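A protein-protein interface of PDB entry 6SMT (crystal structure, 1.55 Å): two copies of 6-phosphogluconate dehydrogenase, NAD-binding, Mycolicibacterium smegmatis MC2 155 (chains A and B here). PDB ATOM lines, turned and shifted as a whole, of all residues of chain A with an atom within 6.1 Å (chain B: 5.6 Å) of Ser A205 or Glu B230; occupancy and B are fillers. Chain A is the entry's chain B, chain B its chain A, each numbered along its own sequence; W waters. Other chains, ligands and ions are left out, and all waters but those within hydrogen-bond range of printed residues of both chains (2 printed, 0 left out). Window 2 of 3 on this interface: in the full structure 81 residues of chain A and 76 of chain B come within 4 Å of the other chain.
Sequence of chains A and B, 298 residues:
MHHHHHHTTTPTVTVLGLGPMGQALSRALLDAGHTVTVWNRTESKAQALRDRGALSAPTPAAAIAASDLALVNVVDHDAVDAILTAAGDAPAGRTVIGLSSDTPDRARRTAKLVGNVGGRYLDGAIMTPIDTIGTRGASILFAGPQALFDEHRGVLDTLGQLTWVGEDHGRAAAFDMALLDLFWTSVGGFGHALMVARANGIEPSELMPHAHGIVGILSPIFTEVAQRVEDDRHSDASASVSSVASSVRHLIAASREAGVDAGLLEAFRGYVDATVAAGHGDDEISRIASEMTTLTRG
The side-chain hydroxyl of Ser A205 is in hydrogen-bond range of the side-chain carboxylate of Glu B230, at 2.9 Å.
NE of Arg A198 is in salt-bridge range of OE2 of Glu A203, at 2.8 Å.
Among the printed residues, pairs that only touch across the chains: Pro A204 with Glu B230, Met A208 with Ala B226, Glu A203 with Glu B230, Pro A204 with Ala B226 and Arg A198 with Val B229.
Ser A205 touches just one residue of chain B: Glu B230.
Glu B230 touches just these residues of chain A: Glu A203 (3.7 Å), Pro A204 (3.5 Å) and Ser A205 (2.9 Å).
Printed residues of chain A within 4 Å of Val B229: Arg A198.
Printed residues of chain B within 4 Å of Met A208: Ala B226 (3.7 Å).
Asp B231 touches none of the printed residues of chain A.
Leu A207 touches none of the printed residues of chain B.
The nearest residue of chain B that does not touch Ser A205 is Ala B226 (5.4 Å).
The nearest residue of chain A that does not touch Glu B230 is Arg A198 (4.1 Å).
Of the 8 printed residues of chain B, 3 touch a printed residue of chain A.
Printed residues of chain B that touch a printed residue of chain A: Ala B226, Val B229 and Glu B230.
Hydrophobic or aromatic side chains of chain A that line the printed part of chain B: Pro A204 and Met A208.
Among the printed residues, 6 pairs touch across the chains.
No position is printed for both chains.
Water W1 bridges OE1 of Glu A203 and OE2 of Glu B230.
Water W2 lies within hydrogen-bond range of the backbone carbonyl oxygen of Val B229 (2.9 Å), the guanidinium group of Arg A198 (3.0 Å) and the backbone carbonyl oxygen of Glu B230 (3.2 Å).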
ATOM      1  N   ARG A 198      -4.401  -1.181  -2.809  1.00  0.00           N
ATOM      2  CA  ARG A 198      -4.222   0.241  -2.424  1.00  0.00           C
ATOM      3  C   ARG A 198      -3.363   0.324  -1.181  1.00  0.00           C
ATOM      4  O   ARG A 198      -2.450   1.233  -1.119  1.00  0.00           O
ATOM      5  CB  ARG A 198      -5.565   0.938  -2.229  1.00  0.00           C
ATOM      6  CG  ARG A 198      -5.466   2.355  -1.737  1.00  0.00           C
ATOM      7  CD  ARG A 198      -6.843   2.962  -1.940  1.00  0.00           C
ATOM      8  NE  ARG A 198      -6.887   3.790  -3.111  1.00  0.00           N
ATOM      9  CZ  ARG A 198      -7.935   4.556  -3.418  1.00  0.00           C
ATOM     10  NH1 ARG A 198      -9.031   4.482  -2.688  1.00  0.00           N
ATOM     11  NH2 ARG A 198      -7.807   5.456  -4.344  1.00  0.00           N
ATOM     12  N   GLU A 203      -2.495   1.779  -6.941  1.00  0.00           N
ATOM     13  CA  GLU A 203      -3.814   2.413  -7.158  1.00  0.00           C
ATOM     14  C   GLU A 203      -4.569   1.562  -8.167  1.00  0.00           C
ATOM     15  O   GLU A 203      -3.980   0.818  -8.945  1.00  0.00           O
ATOM     16  CB  GLU A 203      -3.584   3.852  -7.555  1.00  0.00           C
ATOM     17  CG  GLU A 203      -3.148   4.698  -6.344  1.00  0.00           C
ATOM     18  CD  GLU A 203      -4.264   4.834  -5.324  1.00  0.00           C
ATOM     19  OE1 GLU A 203      -5.235   5.536  -5.671  1.00  0.00           O
ATOM     20  OE2 GLU A 203      -4.331   4.090  -4.289  1.00  0.00           O
ATOM     21  N   PRO A 204      -5.914   1.700  -8.198  1.00  0.00           N
ATOM     22  CA  PRO A 204      -6.718   0.887  -9.081  1.00  0.00           C
ATOM     23  C   PRO A 204      -6.277   1.038 -10.521  1.00  0.00           C
ATOM     24  O   PRO A 204      -6.221   0.054 -11.254  1.00  0.00           O
ATOM     25  CB  PRO A 204      -8.150   1.417  -8.811  1.00  0.00           C
ATOM     26  CG  PRO A 204      -8.092   1.824  -7.372  1.00  0.00           C
ATOM     27  CD  PRO A 204      -6.715   2.435  -7.208  1.00  0.00           C
ATOM     28  N   SER A 205      -5.957   2.250 -10.950  1.00  0.00           N
ATOM     29  CA  SER A 205      -5.550   2.464 -12.359  1.00  0.00           C
ATOM     30  C   SER A 205      -4.287   1.675 -12.732  1.00  0.00           C
ATOM     31  O   SER A 205      -4.169   1.281 -13.885  1.00  0.00           O
ATOM     32  CB  SER A 205      -5.355   3.912 -12.680  1.00  0.00           C
ATOM     33  OG  SER A 205      -4.473   4.495 -11.773  1.00  0.00           O
ATOM     34  N   GLU A 206      -3.413   1.451 -11.753  1.00  0.00           N
ATOM     35  CA  GLU A 206      -2.160   0.702 -12.018  1.00  0.00           C
ATOM     36  C   GLU A 206      -2.473  -0.806 -12.012  1.00  0.00           C
ATOM     37  O   GLU A 206      -1.858  -1.568 -12.834  1.00  0.00           O
ATOM     38  CB  GLU A 206      -1.077   1.040 -11.019  1.00  0.00           C
ATOM     39  CG  GLU A 206       0.236   0.416 -11.386  1.00  0.00           C
ATOM     40  CD  GLU A 206       1.375   0.806 -10.459  1.00  0.00           C
ATOM     41  OE1 GLU A 206       1.147   1.282  -9.329  1.00  0.00           O
ATOM     42  OE2 GLU A 206       2.500   0.438 -10.842  1.00  0.00           O
ATOM     43  N   LEU A 207      -3.400  -1.251 -11.198  1.00  0.00           N
ATOM     44  CA  LEU A 207      -3.754  -2.691 -11.204  1.00  0.00           C
ATOM     45  C   LEU A 207      -4.548  -3.105 -12.423  1.00  0.00           C
ATOM     46  O   LEU A 207      -4.420  -4.226 -12.874  1.00  0.00           O
ATOM     47  CB  LEU A 207      -4.577  -2.994  -9.950  1.00  0.00           C
ATOM     48  CG  LEU A 207      -4.752  -4.478  -9.652  1.00  0.00           C
ATOM     49  CD1 LEU A 207      -3.424  -5.098  -9.174  1.00  0.00           C
ATOM     50  CD2 LEU A 207      -5.821  -4.699  -8.631  1.00  0.00           C
ATOM     51  N   MET A 208      -5.357  -2.180 -12.974  1.00  0.00           N
ATOM     52  CA  MET A 208      -6.397  -2.621 -13.905  1.00  0.00           C
ATOM     53  C   MET A 208      -5.886  -3.346 -15.133  1.00  0.00           C
ATOM     54  O   MET A 208      -6.513  -4.313 -15.559  1.00  0.00           O
ATOM     55  CB  MET A 208      -7.278  -1.431 -14.333  1.00  0.00           C
ATOM     56  CG  MET A 208      -8.283  -1.091 -13.334  1.00  0.00           C
ATOM     57  SD  MET A 208      -9.224  -2.531 -12.671  1.00  0.00           S
ATOM     58  CE  MET A 208      -9.985  -3.158 -14.010  1.00  0.00           C
ATOM     59  N   PRO A 209      -4.783  -2.966 -15.834  1.00  0.00           N
ATOM     60  CA  PRO A 209      -4.352  -3.762 -16.984  1.00  0.00           C
ATOM     61  C   PRO A 209      -4.134  -5.219 -16.622  1.00  0.00           C
ATOM     62  O   PRO A 209      -4.442  -6.139 -17.379  1.00  0.00           O
ATOM     63  CB  PRO A 209      -3.118  -3.011 -17.432  1.00  0.00           C
ATOM     64  CG  PRO A 209      -3.264  -1.595 -16.937  1.00  0.00           C
ATOM     65  CD  PRO A 209      -3.993  -1.736 -15.619  1.00  0.00           C
ATOM     66  N   VAL B 225     -15.901   0.247 -11.750  1.00  0.00           N
ATOM     67  CA  VAL B 225     -15.748   0.236 -10.299  1.00  0.00           C
ATOM     68  C   VAL B 225     -14.415   0.870  -9.904  1.00  0.00           C
ATOM     69  O   VAL B 225     -14.345   1.604  -8.931  1.00  0.00           O
ATOM     70  CB  VAL B 225     -15.931  -1.177  -9.738  1.00  0.00           C
ATOM     71  CG1 VAL B 225     -15.441  -1.304  -8.328  1.00  0.00           C
ATOM     72  CG2 VAL B 225     -17.369  -1.658  -9.947  1.00  0.00           C
ATOM     73  N   ALA B 226     -13.350   0.483 -10.572  1.00  0.00           N
ATOM     74  CA  ALA B 226     -12.022   1.012 -10.235  1.00  0.00           C
ATOM     75  C   ALA B 226     -12.023   2.539 -10.372  1.00  0.00           C
ATOM     76  O   ALA B 226     -11.427   3.206  -9.555  1.00  0.00           O
ATOM     77  CB  ALA B 226     -11.032   0.356 -11.152  1.00  0.00           C
ATOM     78  N   GLN B 227     -12.635   3.046 -11.426  1.00  0.00           N
ATOM     79  CA  GLN B 227     -12.638   4.522 -11.656  1.00  0.00           C
ATOM     80  C   GLN B 227     -13.436   5.181 -10.539  1.00  0.00           C
ATOM     81  O   GLN B 227     -13.029   6.200 -10.003  1.00  0.00           O
ATOM     82  CB  GLN B 227     -13.195   4.855 -13.016  1.00  0.00           C
ATOM     83  CG  GLN B 227     -13.077   6.369 -13.301  1.00  0.00           C
ATOM     84  CD  GLN B 227     -11.637   6.817 -13.450  1.00  0.00           C
ATOM     85  OE1 GLN B 227     -11.117   7.705 -12.724  1.00  0.00           O
ATOM     86  NE2 GLN B 227     -10.924   6.142 -14.334  1.00  0.00           N
ATOM     87  N   ARG B 228     -14.567   4.612 -10.152  1.00  0.00           N
ATOM     88  CA  ARG B 228     -15.394   5.154  -9.064  1.00  0.00           C
ATOM     89  C   ARG B 228     -14.655   5.139  -7.739  1.00  0.00           C
ATOM     90  O   ARG B 228     -14.768   6.105  -6.988  1.00  0.00           O
ATOM     91  CB  ARG B 228     -16.721   4.394  -8.967  1.00  0.00           C
ATOM     92  CG  ARG B 228     -17.692   4.706 -10.071  1.00  0.00           C
ATOM     93  CD  ARG B 228     -18.954   3.904  -9.973  1.00  0.00           C
ATOM     94  NE  ARG B 228     -20.077   4.340 -10.721  1.00  0.00           N
ATOM     95  CZ  ARG B 228     -20.969   5.236 -10.314  1.00  0.00           C
ATOM     96  NH1 ARG B 228     -20.753   5.919  -9.191  1.00  0.00           N
ATOM     97  NH2 ARG B 228     -22.040   5.400 -11.062  1.00  0.00           N
ATOM     98  N   VAL B 229     -13.933   4.076  -7.447  1.00  0.00           N
ATOM     99  CA  VAL B 229     -13.139   3.969  -6.192  1.00  0.00           C
ATOM    100  C   VAL B 229     -12.052   5.063  -6.243  1.00  0.00           C
ATOM    101  O   VAL B 229     -11.915   5.779  -5.268  1.00  0.00           O
ATOM    102  CB  VAL B 229     -12.557   2.555  -6.028  1.00  0.00           C
ATOM    103  CG1 VAL B 229     -11.493   2.500  -4.973  1.00  0.00           C
ATOM    104  CG2 VAL B 229     -13.660   1.558  -5.761  1.00  0.00           C
ATOM    105  N   GLU B 230     -11.376   5.251  -7.362  1.00  0.00           N
ATOM    106  CA  GLU B 230     -10.342   6.320  -7.432  1.00  0.00           C
ATOM    107  C   GLU B 230     -10.922   7.723  -7.293  1.00  0.00           C
ATOM    108  O   GLU B 230     -10.292   8.574  -6.621  1.00  0.00           O
ATOM    109  CB  GLU B 230      -9.666   6.209  -8.783  1.00  0.00           C
ATOM    110  CG  GLU B 230      -8.362   5.508  -8.595  1.00  0.00           C
ATOM    111  CD  GLU B 230      -7.572   5.262  -9.865  1.00  0.00           C
ATOM    112  OE1 GLU B 230      -8.084   5.609 -11.007  1.00  0.00           O
ATOM    113  OE2 GLU B 230      -6.473   4.813  -9.712  1.00  0.00           O
ATOM    114  N   ASP B 231     -12.004   8.002  -7.968  1.00  0.00           N
ATOM    115  CA  ASP B 231     -12.758   9.284  -7.961  1.00  0.00           C
ATOM    116  C   ASP B 231     -13.417   9.478  -6.598  1.00  0.00           C
ATOM    117  O   ASP B 231     -13.984  10.540  -6.385  1.00  0.00           O
ATOM    118  CB  ASP B 231     -13.780   9.346  -9.107  1.00  0.00           C
ATOM    119  CG  ASP B 231     -13.167   9.423 -10.496  1.00  0.00           C
ATOM    120  OD1 ASP B 231     -11.970   9.619 -10.559  1.00  0.00           O
ATOM    121  OD2 ASP B 231     -13.898   9.329 -11.501  1.00  0.00           O
ATOM    122  N   ASP B 232     -13.566   8.444  -5.780  1.00  0.00           N
ATOM    123  CA  ASP B 232     -14.508   8.442  -4.634  1.00  0.00           C
ATOM    124  C   ASP B 232     -15.907   8.903  -5.063  1.00  0.00           C
ATOM    125  O   ASP B 232     -16.508   9.770  -4.370  1.00  0.00           O
ATOM    126  CB  ASP B 232     -13.946   9.323  -3.506  1.00  0.00           C
ATOM    127  CG  ASP B 232     -14.719   9.204  -2.214  1.00  0.00           C
ATOM    128  OD1 ASP B 232     -15.375   8.163  -2.011  1.00  0.00           O
ATOM    129  OD2 ASP B 232     -14.683  10.189  -1.439  1.00  0.00           O
HETATM  130  O   HOH W   1      -5.399   7.103  -7.573  1.00  0.00           O
HETATM  131  O   HOH W   2     -10.113   7.324  -3.673  1.00  0.00           O
